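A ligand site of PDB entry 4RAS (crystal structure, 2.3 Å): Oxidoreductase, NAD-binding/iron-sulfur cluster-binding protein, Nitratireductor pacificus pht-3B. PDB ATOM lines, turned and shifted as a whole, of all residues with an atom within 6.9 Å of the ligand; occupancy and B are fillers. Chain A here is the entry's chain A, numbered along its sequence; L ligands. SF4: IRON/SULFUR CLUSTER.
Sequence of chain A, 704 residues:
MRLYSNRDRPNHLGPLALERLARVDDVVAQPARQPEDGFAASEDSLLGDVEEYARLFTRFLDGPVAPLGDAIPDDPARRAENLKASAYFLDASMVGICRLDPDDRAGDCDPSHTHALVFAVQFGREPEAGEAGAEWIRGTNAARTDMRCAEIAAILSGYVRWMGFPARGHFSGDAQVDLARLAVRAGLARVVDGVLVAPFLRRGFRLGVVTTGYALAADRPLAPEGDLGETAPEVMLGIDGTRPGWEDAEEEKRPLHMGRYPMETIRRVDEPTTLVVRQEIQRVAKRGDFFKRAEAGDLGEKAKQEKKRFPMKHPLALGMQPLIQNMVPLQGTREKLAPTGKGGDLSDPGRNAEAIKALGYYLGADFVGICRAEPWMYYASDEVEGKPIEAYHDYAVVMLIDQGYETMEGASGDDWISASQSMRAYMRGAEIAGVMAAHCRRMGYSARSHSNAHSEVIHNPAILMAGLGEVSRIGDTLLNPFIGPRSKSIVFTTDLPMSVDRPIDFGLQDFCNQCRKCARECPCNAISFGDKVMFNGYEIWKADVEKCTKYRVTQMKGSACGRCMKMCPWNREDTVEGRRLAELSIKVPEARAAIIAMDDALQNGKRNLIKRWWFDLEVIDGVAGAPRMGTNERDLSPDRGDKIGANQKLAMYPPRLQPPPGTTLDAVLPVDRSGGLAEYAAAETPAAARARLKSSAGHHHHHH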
ATOM      1  N   SER A 472      15.929 -16.947   9.965  1.00  0.00           N
ATOM      2  CA  SER A 472      16.128 -17.773  11.187  1.00  0.00           C
ATOM      3  C   SER A 472      14.832 -17.900  11.938  1.00  0.00           C
ATOM      4  O   SER A 472      13.910 -17.111  11.706  1.00  0.00           O
ATOM      5  CB  SER A 472      17.146 -17.122  12.111  1.00  0.00           C
ATOM      6  OG  SER A 472      16.613 -15.949  12.740  1.00  0.00           O
ATOM      7  N   ARG A 473      14.814 -18.806  12.911  1.00  0.00           N
ATOM      8  CA  ARG A 473      13.600 -19.022  13.751  1.00  0.00           C
ATOM      9  C   ARG A 473      13.192 -17.777  14.522  1.00  0.00           C
ATOM     10  O   ARG A 473      12.034 -17.555  14.752  1.00  0.00           O
ATOM     11  CB  ARG A 473      13.810 -20.167  14.761  1.00  0.00           C
ATOM     12  CG  ARG A 473      12.653 -20.468  15.619  1.00  0.00           C
ATOM     13  CD  ARG A 473      12.896 -21.694  16.466  1.00  0.00           C
ATOM     14  NE  ARG A 473      13.111 -22.924  15.724  1.00  0.00           N
ATOM     15  CZ  ARG A 473      12.154 -23.585  15.094  1.00  0.00           C
ATOM     16  NH1 ARG A 473      10.866 -23.194  15.187  1.00  0.00           N
ATOM     17  NH2 ARG A 473      12.473 -24.648  14.320  1.00  0.00           N
ATOM     18  N   ILE A 474      14.125 -16.981  14.919  1.00  0.00           N
ATOM     19  CA  ILE A 474      13.831 -15.818  15.692  1.00  0.00           C
ATOM     20  C   ILE A 474      12.716 -14.998  14.999  1.00  0.00           C
ATOM     21  O   ILE A 474      11.839 -14.485  15.656  1.00  0.00           O
ATOM     22  CB  ILE A 474      15.095 -14.994  15.868  1.00  0.00           C
ATOM     23  CG1 ILE A 474      16.010 -15.693  16.808  1.00  0.00           C
ATOM     24  CG2 ILE A 474      14.788 -13.657  16.461  1.00  0.00           C
ATOM     25  CD1 ILE A 474      17.374 -15.110  16.914  1.00  0.00           C
ATOM     26  N   GLY A 475      12.775 -14.841  13.688  1.00  0.00           N
ATOM     27  CA  GLY A 475      11.571 -14.502  12.969  1.00  0.00           C
ATOM     28  C   GLY A 475      11.785 -13.292  12.087  1.00  0.00           C
ATOM     29  O   GLY A 475      11.934 -13.432  10.902  1.00  0.00           O
ATOM     30  N   THR A 477      14.348 -11.446  12.365  1.00  0.00           N
ATOM     31  CA  THR A 477      15.778 -11.198  12.423  1.00  0.00           C
ATOM     32  C   THR A 477      16.471 -12.218  11.562  1.00  0.00           C
ATOM     33  O   THR A 477      16.217 -13.423  11.689  1.00  0.00           O
ATOM     34  CB  THR A 477      16.308 -11.392  13.856  1.00  0.00           C
ATOM     35  OG1 THR A 477      15.562 -10.529  14.713  1.00  0.00           O
ATOM     36  CG2 THR A 477      17.769 -11.098  13.969  1.00  0.00           C
ATOM     37  N   LEU A 479      20.114 -14.018  10.287  1.00  0.00           N
ATOM     38  CA  LEU A 479      21.263 -14.486  11.004  1.00  0.00           C
ATOM     39  C   LEU A 479      22.436 -14.644  10.017  1.00  0.00           C
ATOM     40  O   LEU A 479      22.299 -15.199   8.908  1.00  0.00           O
ATOM     41  CB  LEU A 479      20.825 -15.769  11.637  1.00  0.00           C
ATOM     42  CG  LEU A 479      21.696 -16.371  12.691  1.00  0.00           C
ATOM     43  CD1 LEU A 479      20.900 -17.365  13.534  1.00  0.00           C
ATOM     44  CD2 LEU A 479      22.865 -17.084  12.059  1.00  0.00           C
ATOM     45  N   PRO A 485      22.911 -13.589  14.911  1.00  0.00           N
ATOM     46  CA  PRO A 485      21.837 -12.613  14.914  1.00  0.00           C
ATOM     47  C   PRO A 485      22.187 -11.387  15.688  1.00  0.00           C
ATOM     48  O   PRO A 485      21.330 -10.548  15.905  1.00  0.00           O
ATOM     49  CB  PRO A 485      20.703 -13.351  15.634  1.00  0.00           C
ATOM     50  CG  PRO A 485      21.444 -14.175  16.686  1.00  0.00           C
ATOM     51  CD  PRO A 485      22.770 -14.537  16.045  1.00  0.00           C
ATOM     52  N   LEU A 508      21.513 -22.867   7.314  1.00  0.00           N
ATOM     53  CA  LEU A 508      20.771 -22.450   8.494  1.00  0.00           C
ATOM     54  C   LEU A 508      19.410 -23.059   8.567  1.00  0.00           C
ATOM     55  O   LEU A 508      18.912 -23.310   9.656  1.00  0.00           O
ATOM     56  CB  LEU A 508      20.653 -20.941   8.576  1.00  0.00           C
ATOM     57  CG  LEU A 508      20.118 -20.452   9.933  1.00  0.00           C
ATOM     58  CD1 LEU A 508      21.121 -20.700  11.048  1.00  0.00           C
ATOM     59  CD2 LEU A 508      19.850 -18.969   9.815  1.00  0.00           C
ATOM     60  N   PHE A 511      19.649 -26.158  10.434  1.00  0.00           N
ATOM     61  CA  PHE A 511      20.105 -25.995  11.796  1.00  0.00           C
ATOM     62  C   PHE A 511      18.961 -25.518  12.685  1.00  0.00           C
ATOM     63  O   PHE A 511      18.675 -26.139  13.652  1.00  0.00           O
ATOM     64  CB  PHE A 511      21.190 -24.980  11.824  1.00  0.00           C
ATOM     65  CG  PHE A 511      21.942 -24.926  13.115  1.00  0.00           C
ATOM     66  CD1 PHE A 511      21.401 -24.342  14.197  1.00  0.00           C
ATOM     67  CD2 PHE A 511      23.222 -25.413  13.197  1.00  0.00           C
ATOM     68  CE1 PHE A 511      22.089 -24.239  15.367  1.00  0.00           C
ATOM     69  CE2 PHE A 511      23.931 -25.332  14.377  1.00  0.00           C
ATOM     70  CZ  PHE A 511      23.368 -24.741  15.457  1.00  0.00           C
ATOM     71  N   CYS A 512      18.259 -24.470  12.243  1.00  0.00           N
ATOM     72  CA  CYS A 512      17.128 -23.905  12.978  1.00  0.00           C
ATOM     73  C   CYS A 512      16.008 -24.885  13.070  1.00  0.00           C
ATOM     74  O   CYS A 512      15.230 -24.863  14.001  1.00  0.00           O
ATOM     75  CB  CYS A 512      16.607 -22.581  12.383  1.00  0.00           C
ATOM     76  SG  CYS A 512      17.513 -21.149  12.800  1.00  0.00           S
ATOM     77  N   ASN A 513      15.909 -25.777  12.133  1.00  0.00           N
ATOM     78  CA  ASN A 513      14.929 -26.827  12.259  1.00  0.00           C
ATOM     79  C   ASN A 513      15.163 -27.804  13.412  1.00  0.00           C
ATOM     80  O   ASN A 513      14.239 -28.409  13.902  1.00  0.00           O
ATOM     81  CB  ASN A 513      14.965 -27.590  11.026  1.00  0.00           C
ATOM     82  CG  ASN A 513      13.640 -27.668  10.453  1.00  0.00           C
ATOM     83  OD1 ASN A 513      13.099 -26.668   9.936  1.00  0.00           O
ATOM     84  ND2 ASN A 513      13.055 -28.870  10.541  1.00  0.00           N
ATOM     85  N   GLN A 514      16.384 -27.921  13.896  1.00  0.00           N
ATOM     86  CA  GLN A 514      16.689 -28.839  15.037  1.00  0.00           C
ATOM     87  C   GLN A 514      16.890 -28.118  16.341  1.00  0.00           C
ATOM     88  O   GLN A 514      17.207 -28.732  17.292  1.00  0.00           O
ATOM     89  CB  GLN A 514      17.956 -29.567  14.680  1.00  0.00           C
ATOM     90  CG  GLN A 514      17.776 -30.353  13.393  1.00  0.00           C
ATOM     91  CD  GLN A 514      19.052 -31.100  13.005  1.00  0.00           C
ATOM     92  OE1 GLN A 514      19.436 -32.033  13.638  1.00  0.00           O
ATOM     93  NE2 GLN A 514      19.662 -30.703  11.902  1.00  0.00           N
ATOM     94  N   CYS A 515      16.821 -26.774  16.365  1.00  0.00           N
ATOM     95  CA  CYS A 515      17.142 -25.999  17.539  1.00  0.00           C
ATOM     96  C   CYS A 515      15.836 -25.297  17.962  1.00  0.00           C
ATOM     97  O   CYS A 515      14.987 -24.949  17.103  1.00  0.00           O
ATOM     98  CB  CYS A 515      18.237 -25.000  17.155  1.00  0.00           C
ATOM     99  SG  CYS A 515      18.800 -23.845  18.438  1.00  0.00           S
ATOM    100  N   ARG A 516      15.701 -24.999  19.219  1.00  0.00           N
ATOM    101  CA  ARG A 516      14.579 -24.222  19.748  1.00  0.00           C
ATOM    102  C   ARG A 516      15.017 -23.267  20.809  1.00  0.00           C
ATOM    103  O   ARG A 516      14.231 -22.790  21.609  1.00  0.00           O
ATOM    104  CB  ARG A 516      13.540 -25.150  20.370  1.00  0.00           C
ATOM    105  CG  ARG A 516      12.871 -26.100  19.386  1.00  0.00           C
ATOM    106  CD  ARG A 516      11.969 -25.430  18.355  1.00  0.00           C
ATOM    107  NE  ARG A 516      11.259 -26.395  17.478  1.00  0.00           N
ATOM    108  CZ  ARG A 516      11.819 -27.091  16.480  1.00  0.00           C
ATOM    109  NH1 ARG A 516      13.100 -26.952  16.201  1.00  0.00           N
ATOM    110  NH2 ARG A 516      11.076 -27.831  15.727  1.00  0.00           N
ATOM    111  N   LYS A 517      16.284 -22.972  20.851  1.00  0.00           N
ATOM    112  CA  LYS A 517      16.783 -22.258  22.031  1.00  0.00           C
ATOM    113  C   LYS A 517      16.217 -20.855  22.171  1.00  0.00           C
ATOM    114  O   LYS A 517      15.772 -20.474  23.255  1.00  0.00           O
ATOM    115  CB  LYS A 517      18.288 -22.277  21.975  1.00  0.00           C
ATOM    116  CG  LYS A 517      18.908 -21.610  23.168  1.00  0.00           C
ATOM    117  CD  LYS A 517      20.274 -22.153  23.472  1.00  0.00           C
ATOM    118  CE  LYS A 517      20.964 -21.470  24.670  1.00  0.00           C
ATOM    119  NZ  LYS A 517      22.177 -22.289  25.027  1.00  0.00           N
ATOM    120  N   CYS A 518      16.246 -20.067  21.070  1.00  0.00           N
ATOM    121  CA  CYS A 518      15.711 -18.704  21.069  1.00  0.00           C
ATOM    122  C   CYS A 518      14.248 -18.772  21.503  1.00  0.00           C
ATOM    123  O   CYS A 518      13.810 -18.021  22.351  1.00  0.00           O
ATOM    124  CB  CYS A 518      15.808 -18.059  19.682  1.00  0.00           C
ATOM    125  SG  CYS A 518      15.090 -19.073  18.340  1.00  0.00           S
ATOM    126  N   ALA A 519      13.491 -19.687  20.938  1.00  0.00           N
ATOM    127  CA  ALA A 519      12.083 -19.813  21.301  1.00  0.00           C
ATOM    128  C   ALA A 519      11.925 -20.103  22.779  1.00  0.00           C
ATOM    129  O   ALA A 519      11.022 -19.604  23.402  1.00  0.00           O
ATOM    130  CB  ALA A 519      11.392 -20.918  20.506  1.00  0.00           C
ATOM    131  N   ILE A 527       8.329 -16.351  19.960  1.00  0.00           N
ATOM    132  CA  ILE A 527       9.055 -16.988  18.885  1.00  0.00           C
ATOM    133  C   ILE A 527       8.507 -18.366  18.633  1.00  0.00           C
ATOM    134  O   ILE A 527       8.187 -19.081  19.601  1.00  0.00           O
ATOM    135  CB  ILE A 527      10.524 -17.034  19.217  1.00  0.00           C
ATOM    136  CG1 ILE A 527      11.094 -15.661  19.220  1.00  0.00           C
ATOM    137  CG2 ILE A 527      11.293 -17.829  18.185  1.00  0.00           C
ATOM    138  CD1 ILE A 527      12.525 -15.645  19.573  1.00  0.00           C
ATOM    139  N   TRP A 541       9.660 -18.046   9.575  1.00  0.00           N
ATOM    140  CA  TRP A 541       9.158 -18.519  10.911  1.00  0.00           C
ATOM    141  C   TRP A 541       8.599 -17.243  11.475  1.00  0.00           C
ATOM    142  O   TRP A 541       9.351 -16.316  11.649  1.00  0.00           O
ATOM    143  CB  TRP A 541      10.307 -19.003  11.777  1.00  0.00           C
ATOM    144  CG  TRP A 541      10.703 -20.395  11.618  1.00  0.00           C
ATOM    145  CD1 TRP A 541      10.044 -21.504  12.100  1.00  0.00           C
ATOM    146  CD2 TRP A 541      11.882 -20.895  11.000  1.00  0.00           C
ATOM    147  NE1 TRP A 541      10.746 -22.633  11.834  1.00  0.00           N
ATOM    148  CE2 TRP A 541      11.909 -22.269  11.212  1.00  0.00           C
ATOM    149  CE3 TRP A 541      12.961 -20.302  10.408  1.00  0.00           C
ATOM    150  CZ2 TRP A 541      12.900 -23.054  10.745  1.00  0.00           C
ATOM    151  CZ3 TRP A 541      13.963 -21.061   9.993  1.00  0.00           C
ATOM    152  CH2 TRP A 541      13.931 -22.438  10.122  1.00  0.00           C
ATOM    153  N   CYS A 564      16.746 -13.085  22.553  1.00  0.00           N
ATOM    154  CA  CYS A 564      16.783 -14.109  21.514  1.00  0.00           C
ATOM    155  C   CYS A 564      18.118 -14.071  20.839  1.00  0.00           C
ATOM    156  O   CYS A 564      18.734 -15.075  20.678  1.00  0.00           O
ATOM    157  CB  CYS A 564      15.674 -13.858  20.533  1.00  0.00           C
ATOM    158  SG  CYS A 564      15.280 -12.114  20.174  1.00  0.00           S
ATOM    159  N   MET A 567      20.848 -15.733  23.144  1.00  0.00           N
ATOM    160  CA  MET A 567      20.810 -17.161  23.510  1.00  0.00           C
ATOM    161  C   MET A 567      21.097 -18.067  22.282  1.00  0.00           C
ATOM    162  O   MET A 567      21.254 -19.261  22.393  1.00  0.00           O
ATOM    163  CB  MET A 567      19.436 -17.513  24.101  1.00  0.00           C
ATOM    164  CG  MET A 567      19.078 -16.797  25.402  1.00  0.00           C
ATOM    165  SD  MET A 567      20.080 -17.336  26.860  1.00  0.00           S
ATOM    166  CE  MET A 567      20.699 -15.740  27.040  1.00  0.00           C
ATOM    167  N   CYS A 568      21.224 -17.466  21.134  1.00  0.00           N
ATOM    168  CA  CYS A 568      21.401 -18.227  19.920  1.00  0.00           C
ATOM    169  C   CYS A 568      22.791 -18.757  19.944  1.00  0.00           C
ATOM    170  O   CYS A 568      23.748 -18.035  20.177  1.00  0.00           O
ATOM    171  CB  CYS A 568      21.230 -17.314  18.675  1.00  0.00           C
ATOM    172  SG  CYS A 568      21.246 -18.312  17.125  1.00  0.00           S
ATOM    173  N   PRO A 569      22.969 -20.013  19.591  1.00  0.00           N
ATOM    174  CA  PRO A 569      24.293 -20.627  19.556  1.00  0.00           C
ATOM    175  C   PRO A 569      25.202 -19.962  18.577  1.00  0.00           C
ATOM    176  O   PRO A 569      26.379 -20.065  18.718  1.00  0.00           O
ATOM    177  CB  PRO A 569      24.001 -22.054  19.053  1.00  0.00           C
ATOM    178  CG  PRO A 569      22.624 -22.307  19.430  1.00  0.00           C
ATOM    179  CD  PRO A 569      21.917 -20.963  19.338  1.00  0.00           C
ATOM    180  N   TRP A 570      24.666 -19.388  17.510  1.00  0.00           N
ATOM    181  CA  TRP A 570      25.576 -18.664  16.606  1.00  0.00           C
ATOM    182  C   TRP A 570      26.104 -17.367  17.113  1.00  0.00           C
ATOM    183  O   TRP A 570      27.006 -16.827  16.538  1.00  0.00           O
ATOM    184  CB  TRP A 570      24.904 -18.359  15.283  1.00  0.00           C
ATOM    185  CG  TRP A 570      24.481 -19.576  14.546  1.00  0.00           C
ATOM    186  CD1 TRP A 570      23.369 -20.302  14.766  1.00  0.00           C
ATOM    187  CD2 TRP A 570      25.142 -20.150  13.462  1.00  0.00           C
ATOM    188  NE1 TRP A 570      23.325 -21.354  13.911  1.00  0.00           N
ATOM    189  CE2 TRP A 570      24.406 -21.276  13.075  1.00  0.00           C
ATOM    190  CE3 TRP A 570      26.318 -19.860  12.775  1.00  0.00           C
ATOM    191  CZ2 TRP A 570      24.753 -22.077  11.998  1.00  0.00           C
ATOM    192  CZ3 TRP A 570      26.664 -20.677  11.717  1.00  0.00           C
ATOM    193  CH2 TRP A 570      25.884 -21.790  11.349  1.00  0.00           C
ATOM    194  N   ASN A 571      25.543 -16.846  18.190  1.00  0.00           N
ATOM    195  CA  ASN A 571      26.155 -15.721  18.871  1.00  0.00           C
ATOM    196  C   ASN A 571      27.346 -16.190  19.731  1.00  0.00           C
ATOM    197  O   ASN A 571      27.187 -16.768  20.828  1.00  0.00           O
ATOM    198  CB  ASN A 571      25.081 -14.983  19.681  1.00  0.00           C
ATOM    199  CG  ASN A 571      25.630 -13.940  20.625  1.00  0.00           C
ATOM    200  OD1 ASN A 571      26.577 -13.298  20.339  1.00  0.00           O
ATOM    201  ND2 ASN A 571      25.067 -13.855  21.752  1.00  0.00           N
ATOM    202  N   ILE A 596      23.997 -28.339  18.810  1.00  0.00           N
ATOM    203  CA  ILE A 596      22.837 -27.732  19.446  1.00  0.00           C
ATOM    204  C   ILE A 596      22.689 -28.214  20.922  1.00  0.00           C
ATOM    205  O   ILE A 596      22.501 -27.390  21.818  1.00  0.00           O
ATOM    206  CB  ILE A 596      21.586 -28.063  18.650  1.00  0.00           C
ATOM    207  CG1 ILE A 596      21.594 -27.238  17.400  1.00  0.00           C
ATOM    208  CG2 ILE A 596      20.322 -27.826  19.477  1.00  0.00           C
ATOM    209  CD1 ILE A 596      20.720 -27.809  16.279  1.00  0.00           C
HETATM  210 FE1  SF4 L   1      16.880 -19.814  17.158  1.00  0.00          FE
HETATM  211 FE2  SF4 L   1      18.567 -21.885  17.319  1.00  0.00          FE
HETATM  212 FE3  SF4 L   1      19.417 -19.493  16.682  1.00  0.00          FE
HETATM  213 FE4  SF4 L   1      18.031 -20.782  14.982  1.00  0.00          FE
HETATM  214  S1  SF4 L   1      19.939 -21.355  15.726  1.00  0.00           S
HETATM  215  S2  SF4 L   1      17.797 -18.762  15.563  1.00  0.00           S
HETATM  216  S3  SF4 L   1      16.695 -21.720  16.319  1.00  0.00           S
HETATM  217  S4  SF4 L   1      18.479 -20.136  18.513  1.00  0.00           S
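An iron atom (FE3) of the ligand is bound by the side-chain sulfur of Cys 568 (2.2 Å). SG of Cys 515 is bound to FE2 of the ligand, 2.3 Å away. N of Cys 518 lies close to S4 of the ligand (3.4 Å). An iron atom (FE1) of the ligand is bound by the side-chain sulfur (SG) of Cys 518, 2.3 Å away. FE4 of the ligand is bound by SG of Cys 512, 2.3 Å away.
N of Trp 570 sits close to SG of Cys 568, 3.6 Å away. The backbone carbonyl oxygen (O) of Cys 515 is in hydrogen-bond range of the guanidinium group (NE) of Arg 473 (3.1 Å). The side-chain sulfur (SG) of Cys 515 sits close to the backbone NH (N) of Lys 517. The backbone carbonyl oxygen (O) of Cys 512 sits at hydrogen-bond distance from the guanidinium group (NH2) of Arg 473. The backbone NH of Ile 474 sits close to the side-chain hydroxyl of Ser 472 (3.5 Å). The backbone carbonyl oxygen (O) of Thr 477 sits at hydrogen-bond distance from the side-chain hydroxyl (OG) of Ser 472 (2.8 Å).
Ser 472 touches the ligand (CB to S2, 3.9 Å). Arg 473 touches the ligand. CG1 of Ile 474 touches S2 of the ligand, 3.8 Å away. Leu 479 touches the ligand. Phe 511 touches the ligand. CD of Pro 569 touches S4 of the ligand, at 3.6 Å. Trp 570 touches the ligand (CD1 to S1, 3.7 Å). Of the 26 residues printed, 11 come within 4 Å of the ligand. The nearest printed residue that does not touch the ligand is Lys 517 (4.1 Å).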
